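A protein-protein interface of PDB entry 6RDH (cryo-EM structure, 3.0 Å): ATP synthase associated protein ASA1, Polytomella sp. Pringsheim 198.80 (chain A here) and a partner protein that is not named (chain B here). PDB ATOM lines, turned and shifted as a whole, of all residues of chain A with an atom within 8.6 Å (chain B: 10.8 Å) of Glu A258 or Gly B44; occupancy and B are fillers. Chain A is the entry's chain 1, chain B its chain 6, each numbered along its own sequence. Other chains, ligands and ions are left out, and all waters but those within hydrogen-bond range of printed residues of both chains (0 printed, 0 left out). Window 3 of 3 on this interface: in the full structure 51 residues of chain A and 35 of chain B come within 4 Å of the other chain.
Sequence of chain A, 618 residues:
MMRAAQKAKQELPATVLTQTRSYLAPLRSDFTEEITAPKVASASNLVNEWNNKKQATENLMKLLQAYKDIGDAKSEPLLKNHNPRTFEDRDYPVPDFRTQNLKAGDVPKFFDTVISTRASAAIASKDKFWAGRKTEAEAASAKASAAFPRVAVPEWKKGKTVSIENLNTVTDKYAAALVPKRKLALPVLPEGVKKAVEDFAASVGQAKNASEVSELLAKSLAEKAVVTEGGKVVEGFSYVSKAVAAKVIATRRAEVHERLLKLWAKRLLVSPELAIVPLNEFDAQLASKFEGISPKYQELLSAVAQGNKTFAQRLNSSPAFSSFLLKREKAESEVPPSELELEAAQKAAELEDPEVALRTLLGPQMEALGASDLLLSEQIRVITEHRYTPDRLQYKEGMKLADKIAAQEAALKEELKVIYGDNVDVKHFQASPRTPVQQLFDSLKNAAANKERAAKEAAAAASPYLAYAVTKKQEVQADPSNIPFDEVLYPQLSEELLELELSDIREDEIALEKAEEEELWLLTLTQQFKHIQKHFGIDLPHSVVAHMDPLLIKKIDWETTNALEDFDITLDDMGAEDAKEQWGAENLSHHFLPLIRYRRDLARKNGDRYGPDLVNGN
Glu A258 touches one residue of chain B. Of chain A, only Glu A258 comes within 4 Å of Gly B44. No residue of chain B comes within 4 Å of Ala A254. His A257 touches none of the printed residues of chain B. Of chain B, only Leu B47 comes within 4 Å of Leu A261. No residue of chain A comes within 4 Å of Ala B45. Of the printed residues of chain A, Val B39 touches Lys A262 and Lys A266. Of the printed residues of chain B, Lys A266 touches Val B39 (3.9 Å) and Asn B40 (3.2 Å). Of the printed residues of chain A, Leu B48 touches Met A366. Printed residues of chain B within 4 Å of Met A366: Leu B48 (3.8 Å). Glu A255 touches none of the printed residues of chain B. The nearest residue of chain A that does not touch Gly B44 is Lys A262 (5.6 Å). The nearest printed residue of chain A that does not touch Leu B48 is Leu A261 (4.7 Å).
The side-chain amino group (NZ) of Lys A266 sits close to the side-chain amide nitrogen (ND2) of Asn B40 (3.2 Å). O of Thr B42 sits close to NZ of Lys A262 (3.4 Å). The backbone carbonyl oxygen of Asn B40 lies within hydrogen-bond range of the side-chain amino group of Lys A262, at 3.0 Å.
O of Val B39 lies within hydrogen-bond range of OG1 of Thr B42 (2.7 Å). NE2 of His A257 is in hydrogen-bond range of O of Met A366 (2.8 Å). OE2 of Glu A258 lies within salt-bridge range of NZ of Lys A262 (3.99 Å). The backbone carbonyl oxygen (O) of Ile B36 sits close to the side-chain amide oxygen (OD1) of Asn B40, at 2.9 Å.
Hydrophobic or aromatic side chains of chain B that line the printed part of chain A: Val B39, Leu B47 and Leu B48. Of the 22 printed residues of chain A, 5 touch a printed residue of chain B.
Among the printed residues, merely in contact across the chains: Lys A262 with Val B39 (3.6 Å), Glu A258 with Gly B44 (3.7 Å), Met A366 with Leu B48 (3.8 Å), Leu A261 with Leu B47 (3.9 Å) and Lys A266 with Val B39 (3.9 Å).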
ATOM      1  N   THR A 251     -14.490  12.802  23.522  1.00  0.00           N
ATOM      2  CA  THR A 251     -13.640  12.411  22.398  1.00  0.00           C
ATOM      3  C   THR A 251     -13.998  11.024  21.884  1.00  0.00           C
ATOM      4  O   THR A 251     -13.983  10.782  20.671  1.00  0.00           O
ATOM      5  CB  THR A 251     -12.159  12.453  22.767  1.00  0.00           C
ATOM      6  OG1 THR A 251     -11.861  11.411  23.703  1.00  0.00           O
ATOM      7  CG2 THR A 251     -11.755  13.813  23.303  1.00  0.00           C
ATOM      8  N   ARG A 252     -14.335  10.100  22.789  1.00  0.00           N
ATOM      9  CA  ARG A 252     -14.730   8.764  22.357  1.00  0.00           C
ATOM     10  C   ARG A 252     -16.054   8.785  21.596  1.00  0.00           C
ATOM     11  O   ARG A 252     -16.204   8.097  20.577  1.00  0.00           O
ATOM     12  CB  ARG A 252     -14.804   7.855  23.574  1.00  0.00           C
ATOM     13  CG  ARG A 252     -14.595   6.403  23.297  1.00  0.00           C
ATOM     14  CD  ARG A 252     -13.208   6.098  22.832  1.00  0.00           C
ATOM     15  NE  ARG A 252     -13.053   4.668  22.589  1.00  0.00           N
ATOM     16  CZ  ARG A 252     -13.404   4.056  21.463  1.00  0.00           C
ATOM     17  NH1 ARG A 252     -13.925   4.746  20.465  1.00  0.00           N
ATOM     18  NH2 ARG A 252     -13.226   2.752  21.329  1.00  0.00           N
ATOM     19  N   ARG A 253     -17.005   9.607  22.043  1.00  0.00           N
ATOM     20  CA  ARG A 253     -18.268   9.763  21.328  1.00  0.00           C
ATOM     21  C   ARG A 253     -18.064  10.421  19.978  1.00  0.00           C
ATOM     22  O   ARG A 253     -18.714  10.044  19.002  1.00  0.00           O
ATOM     23  CB  ARG A 253     -19.248  10.594  22.147  1.00  0.00           C
ATOM     24  CG  ARG A 253     -20.219   9.806  22.967  1.00  0.00           C
ATOM     25  CD  ARG A 253     -21.001  10.730  23.856  1.00  0.00           C
ATOM     26  NE  ARG A 253     -21.709  10.018  24.908  1.00  0.00           N
ATOM     27  CZ  ARG A 253     -22.109  10.583  26.040  1.00  0.00           C
ATOM     28  NH1 ARG A 253     -21.864  11.864  26.267  1.00  0.00           N
ATOM     29  NH2 ARG A 253     -22.749   9.868  26.953  1.00  0.00           N
ATOM     30  N   ALA A 254     -17.157  11.396  19.900  1.00  0.00           N
ATOM     31  CA  ALA A 254     -16.917  12.079  18.637  1.00  0.00           C
ATOM     32  C   ALA A 254     -16.253  11.161  17.622  1.00  0.00           C
ATOM     33  O   ALA A 254     -16.605  11.189  16.439  1.00  0.00           O
ATOM     34  CB  ALA A 254     -16.066  13.321  18.870  1.00  0.00           C
ATOM     35  N   GLU A 255     -15.325  10.309  18.062  1.00  0.00           N
ATOM     36  CA  GLU A 255     -14.688   9.427  17.091  1.00  0.00           C
ATOM     37  C   GLU A 255     -15.604   8.282  16.665  1.00  0.00           C
ATOM     38  O   GLU A 255     -15.593   7.898  15.488  1.00  0.00           O
ATOM     39  CB  GLU A 255     -13.351   8.906  17.617  1.00  0.00           C
ATOM     40  CG  GLU A 255     -13.377   8.053  18.850  1.00  0.00           C
ATOM     41  CD  GLU A 255     -12.049   7.363  19.077  1.00  0.00           C
ATOM     42  OE1 GLU A 255     -11.483   6.843  18.094  1.00  0.00           O
ATOM     43  OE2 GLU A 255     -11.560   7.344  20.224  1.00  0.00           O
ATOM     44  N   VAL A 256     -16.450   7.767  17.562  1.00  0.00           N
ATOM     45  CA  VAL A 256     -17.405   6.749  17.126  1.00  0.00           C
ATOM     46  C   VAL A 256     -18.487   7.362  16.236  1.00  0.00           C
ATOM     47  O   VAL A 256     -18.947   6.730  15.273  1.00  0.00           O
ATOM     48  CB  VAL A 256     -17.963   6.021  18.360  1.00  0.00           C
ATOM     49  CG1 VAL A 256     -19.244   5.283  18.072  1.00  0.00           C
ATOM     50  CG2 VAL A 256     -16.940   5.045  18.846  1.00  0.00           C
ATOM     51  N   HIS A 257     -18.836   8.625  16.464  1.00  0.00           N
ATOM     52  CA  HIS A 257     -19.804   9.273  15.596  1.00  0.00           C
ATOM     53  C   HIS A 257     -19.225   9.574  14.225  1.00  0.00           C
ATOM     54  O   HIS A 257     -19.939   9.480  13.220  1.00  0.00           O
ATOM     55  CB  HIS A 257     -20.305  10.543  16.246  1.00  0.00           C
ATOM     56  CG  HIS A 257     -21.068  11.424  15.322  1.00  0.00           C
ATOM     57  ND1 HIS A 257     -22.327  11.107  14.868  1.00  0.00           N
ATOM     58  CD2 HIS A 257     -20.755  12.618  14.771  1.00  0.00           C
ATOM     59  CE1 HIS A 257     -22.753  12.068  14.071  1.00  0.00           C
ATOM     60  NE2 HIS A 257     -21.821  12.997  13.997  1.00  0.00           N
ATOM     61  N   GLU A 258     -17.934   9.898  14.141  1.00  0.00           N
ATOM     62  CA  GLU A 258     -17.357  10.046  12.812  1.00  0.00           C
ATOM     63  C   GLU A 258     -17.188   8.701  12.129  1.00  0.00           C
ATOM     64  O   GLU A 258     -17.223   8.651  10.901  1.00  0.00           O
ATOM     65  CB  GLU A 258     -16.024  10.795  12.851  1.00  0.00           C
ATOM     66  CG  GLU A 258     -14.789   9.941  12.998  1.00  0.00           C
ATOM     67  CD  GLU A 258     -13.534  10.756  13.171  1.00  0.00           C
ATOM     68  OE1 GLU A 258     -13.641  11.991  13.284  1.00  0.00           O
ATOM     69  OE2 GLU A 258     -12.436  10.164  13.192  1.00  0.00           O
ATOM     70  N   ARG A 259     -17.072   7.603  12.883  1.00  0.00           N
ATOM     71  CA  ARG A 259     -17.104   6.291  12.244  1.00  0.00           C
ATOM     72  C   ARG A 259     -18.481   5.981  11.673  1.00  0.00           C
ATOM     73  O   ARG A 259     -18.590   5.376  10.603  1.00  0.00           O
ATOM     74  CB  ARG A 259     -16.696   5.206  13.223  1.00  0.00           C
ATOM     75  CG  ARG A 259     -15.220   5.071  13.416  1.00  0.00           C
ATOM     76  CD  ARG A 259     -14.941   3.788  14.146  1.00  0.00           C
ATOM     77  NE  ARG A 259     -15.296   2.641  13.329  1.00  0.00           N
ATOM     78  CZ  ARG A 259     -14.408   1.800  12.822  1.00  0.00           C
ATOM     79  NH1 ARG A 259     -14.804   0.780  12.080  1.00  0.00           N
ATOM     80  NH2 ARG A 259     -13.122   1.974  13.075  1.00  0.00           N
ATOM     81  N   LEU A 260     -19.541   6.395  12.365  1.00  0.00           N
ATOM     82  CA  LEU A 260     -20.890   6.207  11.830  1.00  0.00           C
ATOM     83  C   LEU A 260     -21.118   7.048  10.584  1.00  0.00           C
ATOM     84  O   LEU A 260     -21.726   6.582   9.608  1.00  0.00           O
ATOM     85  CB  LEU A 260     -21.928   6.555  12.889  1.00  0.00           C
ATOM     86  CG  LEU A 260     -23.380   6.601  12.426  1.00  0.00           C
ATOM     87  CD1 LEU A 260     -23.959   5.212  12.361  1.00  0.00           C
ATOM     88  CD2 LEU A 260     -24.200   7.480  13.320  1.00  0.00           C
ATOM     89  N   LEU A 261     -20.635   8.288  10.600  1.00  0.00           N
ATOM     90  CA  LEU A 261     -20.754   9.143   9.427  1.00  0.00           C
ATOM     91  C   LEU A 261     -19.946   8.611   8.258  1.00  0.00           C
ATOM     92  O   LEU A 261     -20.397   8.707   7.118  1.00  0.00           O
ATOM     93  CB  LEU A 261     -20.316  10.559   9.761  1.00  0.00           C
ATOM     94  CG  LEU A 261     -21.330  11.414  10.504  1.00  0.00           C
ATOM     95  CD1 LEU A 261     -20.767  12.790  10.685  1.00  0.00           C
ATOM     96  CD2 LEU A 261     -22.596  11.491   9.722  1.00  0.00           C
ATOM     97  N   LYS A 262     -18.784   8.008   8.518  1.00  0.00           N
ATOM     98  CA  LYS A 262     -18.014   7.371   7.455  1.00  0.00           C
ATOM     99  C   LYS A 262     -18.733   6.159   6.885  1.00  0.00           C
ATOM    100  O   LYS A 262     -18.711   5.941   5.669  1.00  0.00           O
ATOM    101  CB  LYS A 262     -16.644   6.962   7.978  1.00  0.00           C
ATOM    102  CG  LYS A 262     -15.658   8.083   8.050  1.00  0.00           C
ATOM    103  CD  LYS A 262     -14.419   7.658   8.778  1.00  0.00           C
ATOM    104  CE  LYS A 262     -13.504   8.833   8.943  1.00  0.00           C
ATOM    105  NZ  LYS A 262     -12.222   8.469   9.584  1.00  0.00           N
ATOM    106  N   LEU A 263     -19.364   5.361   7.754  1.00  0.00           N
ATOM    107  CA  LEU A 263     -20.128   4.192   7.326  1.00  0.00           C
ATOM    108  C   LEU A 263     -21.244   4.582   6.374  1.00  0.00           C
ATOM    109  O   LEU A 263     -21.334   4.079   5.246  1.00  0.00           O
ATOM    110  CB  LEU A 263     -20.722   3.495   8.542  1.00  0.00           C
ATOM    111  CG  LEU A 263     -21.153   2.049   8.375  1.00  0.00           C
ATOM    112  CD1 LEU A 263     -19.949   1.161   8.571  1.00  0.00           C
ATOM    113  CD2 LEU A 263     -22.264   1.681   9.312  1.00  0.00           C
ATOM    114  N   TRP A 264     -22.084   5.516   6.798  1.00  0.00           N
ATOM    115  CA  TRP A 264     -23.175   5.925   5.931  1.00  0.00           C
ATOM    116  C   TRP A 264     -22.699   6.749   4.747  1.00  0.00           C
ATOM    117  O   TRP A 264     -23.378   6.765   3.719  1.00  0.00           O
ATOM    118  CB  TRP A 264     -24.220   6.678   6.733  1.00  0.00           C
ATOM    119  CG  TRP A 264     -25.038   5.767   7.556  1.00  0.00           C
ATOM    120  CD1 TRP A 264     -25.020   5.653   8.901  1.00  0.00           C
ATOM    121  CD2 TRP A 264     -25.989   4.814   7.085  1.00  0.00           C
ATOM    122  NE1 TRP A 264     -25.904   4.695   9.309  1.00  0.00           N
ATOM    123  CE2 TRP A 264     -26.514   4.165   8.207  1.00  0.00           C
ATOM    124  CE3 TRP A 264     -26.447   4.445   5.816  1.00  0.00           C
ATOM    125  CZ2 TRP A 264     -27.475   3.180   8.104  1.00  0.00           C
ATOM    126  CZ3 TRP A 264     -27.401   3.476   5.717  1.00  0.00           C
ATOM    127  CH2 TRP A 264     -27.907   2.850   6.852  1.00  0.00           C
ATOM    128  N   ALA A 265     -21.523   7.372   4.838  1.00  0.00           N
ATOM    129  CA  ALA A 265     -20.960   8.069   3.693  1.00  0.00           C
ATOM    130  C   ALA A 265     -20.580   7.100   2.593  1.00  0.00           C
ATOM    131  O   ALA A 265     -20.879   7.352   1.426  1.00  0.00           O
ATOM    132  CB  ALA A 265     -19.747   8.883   4.115  1.00  0.00           C
ATOM    133  N   LYS A 266     -19.940   5.983   2.947  1.00  0.00           N
ATOM    134  CA  LYS A 266     -19.634   4.956   1.952  1.00  0.00           C
ATOM    135  C   LYS A 266     -20.902   4.372   1.353  1.00  0.00           C
ATOM    136  O   LYS A 266     -21.004   4.210   0.129  1.00  0.00           O
ATOM    137  CB  LYS A 266     -18.818   3.832   2.572  1.00  0.00           C
ATOM    138  CG  LYS A 266     -17.519   4.236   3.163  1.00  0.00           C
ATOM    139  CD  LYS A 266     -17.063   3.163   4.099  1.00  0.00           C
ATOM    140  CE  LYS A 266     -15.950   3.625   4.981  1.00  0.00           C
ATOM    141  NZ  LYS A 266     -15.537   2.517   5.864  1.00  0.00           N
ATOM    142  N   GLN A 365     -29.118  12.478  13.721  1.00  0.00           N
ATOM    143  CA  GLN A 365     -27.914  11.713  13.998  1.00  0.00           C
ATOM    144  C   GLN A 365     -26.684  12.265  13.316  1.00  0.00           C
ATOM    145  O   GLN A 365     -25.652  11.604  13.347  1.00  0.00           O
ATOM    146  CB  GLN A 365     -28.101  10.264  13.575  1.00  0.00           C
ATOM    147  CG  GLN A 365     -29.077   9.508  14.405  1.00  0.00           C
ATOM    148  CD  GLN A 365     -28.731   8.058  14.469  1.00  0.00           C
ATOM    149  OE1 GLN A 365     -27.961   7.632  15.324  1.00  0.00           O
ATOM    150  NE2 GLN A 365     -29.286   7.282  13.558  1.00  0.00           N
ATOM    151  N   MET A 366     -26.765  13.435  12.690  1.00  0.00           N
ATOM    152  CA  MET A 366     -25.616  14.030  12.027  1.00  0.00           C
ATOM    153  C   MET A 366     -24.623  14.624  13.007  1.00  0.00           C
ATOM    154  O   MET A 366     -23.455  14.804  12.658  1.00  0.00           O
ATOM    155  CB  MET A 366     -26.080  15.116  11.064  1.00  0.00           C
ATOM    156  CG  MET A 366     -26.748  14.596   9.818  1.00  0.00           C
ATOM    157  SD  MET A 366     -25.603  13.680   8.784  1.00  0.00           S
ATOM    158  CE  MET A 366     -24.315  14.890   8.565  1.00  0.00           C
ATOM    159  N   GLU A 367     -25.067  14.940  14.213  1.00  0.00           N
ATOM    160  CA  GLU A 367     -24.231  15.470  15.274  1.00  0.00           C
ATOM    161  C   GLU A 367     -24.166  14.452  16.397  1.00  0.00           C
ATOM    162  O   GLU A 367     -25.081  13.645  16.567  1.00  0.00           O
ATOM    163  CB  GLU A 367     -24.792  16.787  15.772  1.00  0.00           C
ATOM    164  CG  GLU A 367     -26.277  16.722  15.967  1.00  0.00           C
ATOM    165  CD  GLU A 367     -26.926  18.082  15.954  1.00  0.00           C
ATOM    166  OE1 GLU A 367     -26.192  19.090  15.895  1.00  0.00           O
ATOM    167  OE2 GLU A 367     -28.172  18.145  15.973  1.00  0.00           O
ATOM    168  N   ALA A 368     -23.086  14.504  17.174  1.00  0.00           N
ATOM    169  CA  ALA A 368     -22.797  13.476  18.161  1.00  0.00           C
ATOM    170  C   ALA A 368     -23.794  13.541  19.316  1.00  0.00           C
ATOM    171  O   ALA A 368     -24.684  14.393  19.363  1.00  0.00           O
ATOM    172  CB  ALA A 368     -21.366  13.621  18.666  1.00  0.00           C
ATOM    173  N   GLU A 509     -19.041   0.880  18.669  1.00  0.00           N
ATOM    174  CA  GLU A 509     -17.904   0.737  17.770  1.00  0.00           C
ATOM    175  C   GLU A 509     -17.694  -0.710  17.353  1.00  0.00           C
ATOM    176  O   GLU A 509     -17.198  -0.963  16.255  1.00  0.00           O
ATOM    177  CB  GLU A 509     -16.643   1.287  18.417  1.00  0.00           C
ATOM    178  CG  GLU A 509     -15.595   1.692  17.417  1.00  0.00           C
ATOM    179  CD  GLU A 509     -14.302   2.095  18.070  1.00  0.00           C
ATOM    180  OE1 GLU A 509     -14.121   1.785  19.262  1.00  0.00           O
ATOM    181  OE2 GLU A 509     -13.460   2.713  17.389  1.00  0.00           O
ATOM    182  N   LEU A 512     -20.099  -1.144  14.528  1.00  0.00           N
ATOM    183  CA  LEU A 512     -19.613  -0.474  13.327  1.00  0.00           C
ATOM    184  C   LEU A 512     -18.401  -1.166  12.724  1.00  0.00           C
ATOM    185  O   LEU A 512     -18.170  -1.059  11.518  1.00  0.00           O
ATOM    186  CB  LEU A 512     -19.282   0.973  13.646  1.00  0.00           C
ATOM    187  CG  LEU A 512     -20.295   2.021  13.227  1.00  0.00           C
ATOM    188  CD1 LEU A 512     -21.679   1.704  13.711  1.00  0.00           C
ATOM    189  CD2 LEU A 512     -19.840   3.296  13.844  1.00  0.00           C
ATOM    190  N   ILE B  36     -13.887   3.524  -0.122  1.00  0.00           N
ATOM    191  CA  ILE B  36     -13.666   3.110   1.258  1.00  0.00           C
ATOM    192  C   ILE B  36     -12.379   3.708   1.798  1.00  0.00           C
ATOM    193  O   ILE B  36     -12.361   4.282   2.893  1.00  0.00           O
ATOM    194  CB  ILE B  36     -13.668   1.575   1.339  1.00  0.00           C
ATOM    195  CG1 ILE B  36     -15.093   1.051   1.247  1.00  0.00           C
ATOM    196  CG2 ILE B  36     -13.010   1.089   2.596  1.00  0.00           C
ATOM    197  CD1 ILE B  36     -15.165  -0.412   1.048  1.00  0.00           C
ATOM    198  N   SER B  38     -10.725   6.405   0.502  1.00  0.00           N
ATOM    199  CA  SER B  38     -10.810   7.857   0.494  1.00  0.00           C
ATOM    200  C   SER B  38     -11.790   8.409   1.515  1.00  0.00           C
ATOM    201  O   SER B  38     -11.740   9.604   1.799  1.00  0.00           O
ATOM    202  CB  SER B  38     -11.200   8.349  -0.893  1.00  0.00           C
ATOM    203  OG  SER B  38     -10.191   8.049  -1.835  1.00  0.00           O
ATOM    204  N   VAL B  39     -12.686   7.595   2.054  1.00  0.00           N
ATOM    205  CA  VAL B  39     -13.527   8.043   3.158  1.00  0.00           C
ATOM    206  C   VAL B  39     -12.847   7.798   4.495  1.00  0.00           C
ATOM    207  O   VAL B  39     -12.898   8.655   5.379  1.00  0.00           O
ATOM    208  CB  VAL B  39     -14.916   7.374   3.071  1.00  0.00           C
ATOM    209  CG1 VAL B  39     -15.692   7.536   4.332  1.00  0.00           C
ATOM    210  CG2 VAL B  39     -15.719   8.019   1.980  1.00  0.00           C
ATOM    211  N   ASN B  40     -12.144   6.668   4.638  1.00  0.00           N
ATOM    212  CA  ASN B  40     -11.531   6.333   5.920  1.00  0.00           C
ATOM    213  C   ASN B  40     -10.412   7.298   6.299  1.00  0.00           C
ATOM    214  O   ASN B  40     -10.256   7.625   7.480  1.00  0.00           O
ATOM    215  CB  ASN B  40     -11.001   4.904   5.909  1.00  0.00           C
ATOM    216  CG  ASN B  40     -12.092   3.881   6.060  1.00  0.00           C
ATOM    217  OD1 ASN B  40     -12.105   2.868   5.374  1.00  0.00           O
ATOM    218  ND2 ASN B  40     -13.031   4.150   6.948  1.00  0.00           N
ATOM    219  N   GLU B  41      -9.621   7.764   5.340  1.00  0.00           N
ATOM    220  CA  GLU B  41      -8.577   8.733   5.677  1.00  0.00           C
ATOM    221  C   GLU B  41      -9.029  10.174   5.452  1.00  0.00           C
ATOM    222  O   GLU B  41      -8.331  10.975   4.843  1.00  0.00           O
ATOM    223  CB  GLU B  41      -7.290   8.423   4.917  1.00  0.00           C
ATOM    224  CG  GLU B  41      -7.383   8.305   3.407  1.00  0.00           C
ATOM    225  CD  GLU B  41      -6.215   7.552   2.803  1.00  0.00           C
ATOM    226  OE1 GLU B  41      -5.684   6.638   3.467  1.00  0.00           O
ATOM    227  OE2 GLU B  41      -5.831   7.871   1.660  1.00  0.00           O
ATOM    228  N   THR B  42     -10.182  10.555   5.992  1.00  0.00           N
ATOM    229  CA  THR B  42     -10.599  11.953   6.032  1.00  0.00           C
ATOM    230  C   THR B  42     -11.091  12.274   7.430  1.00  0.00           C
ATOM    231  O   THR B  42     -11.825  11.482   8.027  1.00  0.00           O
ATOM    232  CB  THR B  42     -11.700  12.267   5.019  1.00  0.00           C
ATOM    233  OG1 THR B  42     -12.766  11.327   5.164  1.00  0.00           O
ATOM    234  CG2 THR B  42     -11.174  12.255   3.607  1.00  0.00           C
ATOM    235  N   SER B  43     -10.692  13.429   7.949  1.00  0.00           N
ATOM    236  CA  SER B  43     -11.161  13.860   9.253  1.00  0.00           C
ATOM    237  C   SER B  43     -12.634  14.243   9.185  1.00  0.00           C
ATOM    238  O   SER B  43     -13.173  14.552   8.121  1.00  0.00           O
ATOM    239  CB  SER B  43     -10.337  15.042   9.752  1.00  0.00           C
ATOM    240  OG  SER B  43     -10.522  16.168   8.918  1.00  0.00           O
ATOM    241  N   GLY B  44     -13.287  14.224  10.347  1.00  0.00           N
ATOM    242  CA  GLY B  44     -14.705  14.521  10.400  1.00  0.00           C
ATOM    243  C   GLY B  44     -15.047  15.964  10.112  1.00  0.00           C
ATOM    244  O   GLY B  44     -16.192  16.256   9.752  1.00  0.00           O
ATOM    245  N   ALA B  45     -14.081  16.874  10.253  1.00  0.00           N
ATOM    246  CA  ALA B  45     -14.343  18.282   9.979  1.00  0.00           C
ATOM    247  C   ALA B  45     -14.511  18.529   8.489  1.00  0.00           C
ATOM    248  O   ALA B  45     -15.332  19.356   8.081  1.00  0.00           O
ATOM    249  CB  ALA B  45     -13.218  19.146  10.540  1.00  0.00           C
ATOM    250  N   ASN B  46     -13.748  17.823   7.667  1.00  0.00           N
ATOM    251  CA  ASN B  46     -13.815  17.953   6.218  1.00  0.00           C
ATOM    252  C   ASN B  46     -14.253  16.654   5.549  1.00  0.00           C
ATOM    253  O   ASN B  46     -13.677  16.229   4.550  1.00  0.00           O
ATOM    254  CB  ASN B  46     -12.479  18.441   5.666  1.00  0.00           C
ATOM    255  CG  ASN B  46     -11.305  17.606   6.134  1.00  0.00           C
ATOM    256  OD1 ASN B  46     -11.469  16.571   6.777  1.00  0.00           O
ATOM    257  ND2 ASN B  46     -10.100  18.073   5.831  1.00  0.00           N
ATOM    258  N   LEU B  47     -15.270  16.001   6.111  1.00  0.00           N
ATOM    259  CA  LEU B  47     -15.862  14.847   5.449  1.00  0.00           C
ATOM    260  C   LEU B  47     -16.939  15.273   4.468  1.00  0.00           C
ATOM    261  O   LEU B  47     -16.897  14.897   3.296  1.00  0.00           O
ATOM    262  CB  LEU B  47     -16.453  13.885   6.472  1.00  0.00           C
ATOM    263  CG  LEU B  47     -17.124  12.648   5.884  1.00  0.00           C
ATOM    264  CD1 LEU B  47     -16.082  11.650   5.482  1.00  0.00           C
ATOM    265  CD2 LEU B  47     -18.086  12.034   6.858  1.00  0.00           C
ATOM    266  N   LEU B  48     -17.909  16.063   4.924  1.00  0.00           N
ATOM    267  CA  LEU B  48     -19.026  16.414   4.057  1.00  0.00           C
ATOM    268  C   LEU B  48     -18.633  17.408   2.977  1.00  0.00           C
ATOM    269  O   LEU B  48     -19.315  17.507   1.957  1.00  0.00           O
ATOM    270  CB  LEU B  48     -20.194  16.966   4.867  1.00  0.00           C
ATOM    271  CG  LEU B  48     -21.121  15.933   5.508  1.00  0.00           C
ATOM    272  CD1 LEU B  48     -20.586  15.386   6.814  1.00  0.00           C
ATOM    273  CD2 LEU B  48     -22.514  16.485   5.671  1.00  0.00           C
ATOM    274  N   SER B  49     -17.547  18.149   3.168  1.00  0.00           N
ATOM    275  CA  SER B  49     -17.033  18.942   2.062  1.00  0.00           C
ATOM    276  C   SER B  49     -16.395  18.053   1.011  1.00  0.00           C
ATOM    277  O   SER B  49     -16.540  18.306  -0.189  1.00  0.00           O
ATOM    278  CB  SER B  49     -16.023  19.963   2.571  1.00  0.00           C
ATOM    279  OG  SER B  49     -14.874  19.311   3.084  1.00  0.00           O
ATOM    280  N   SER B  50     -15.716  16.998   1.439  1.00  0.00           N
ATOM    281  CA  SER B  50     -14.966  16.146   0.537  1.00  0.00           C
ATOM    282  C   SER B  50     -15.809  15.079  -0.133  1.00  0.00           C
ATOM    283  O   SER B  50     -15.252  14.270  -0.873  1.00  0.00           O
ATOM    284  CB  SER B  50     -13.826  15.465   1.289  1.00  0.00           C
ATOM    285  OG  SER B  50     -13.152  14.557   0.444  1.00  0.00           O
ATOM    286  N   LEU B  51     -17.121  15.045   0.093  1.00  0.00           N
ATOM    287  CA  LEU B  51     -17.905  13.919  -0.395  1.00  0.00           C
ATOM    288  C   LEU B  51     -18.144  13.983  -1.892  1.00  0.00           C
ATOM    289  O   LEU B  51     -18.200  12.936  -2.541  1.00  0.00           O
ATOM    290  CB  LEU B  51     -19.239  13.842   0.338  1.00  0.00           C
ATOM    291  CG  LEU B  51     -19.245  13.126   1.687  1.00  0.00           C
ATOM    292  CD1 LEU B  51     -20.663  12.874   2.126  1.00  0.00           C
ATOM    293  CD2 LEU B  51     -18.471  11.834   1.615  1.00  0.00           C
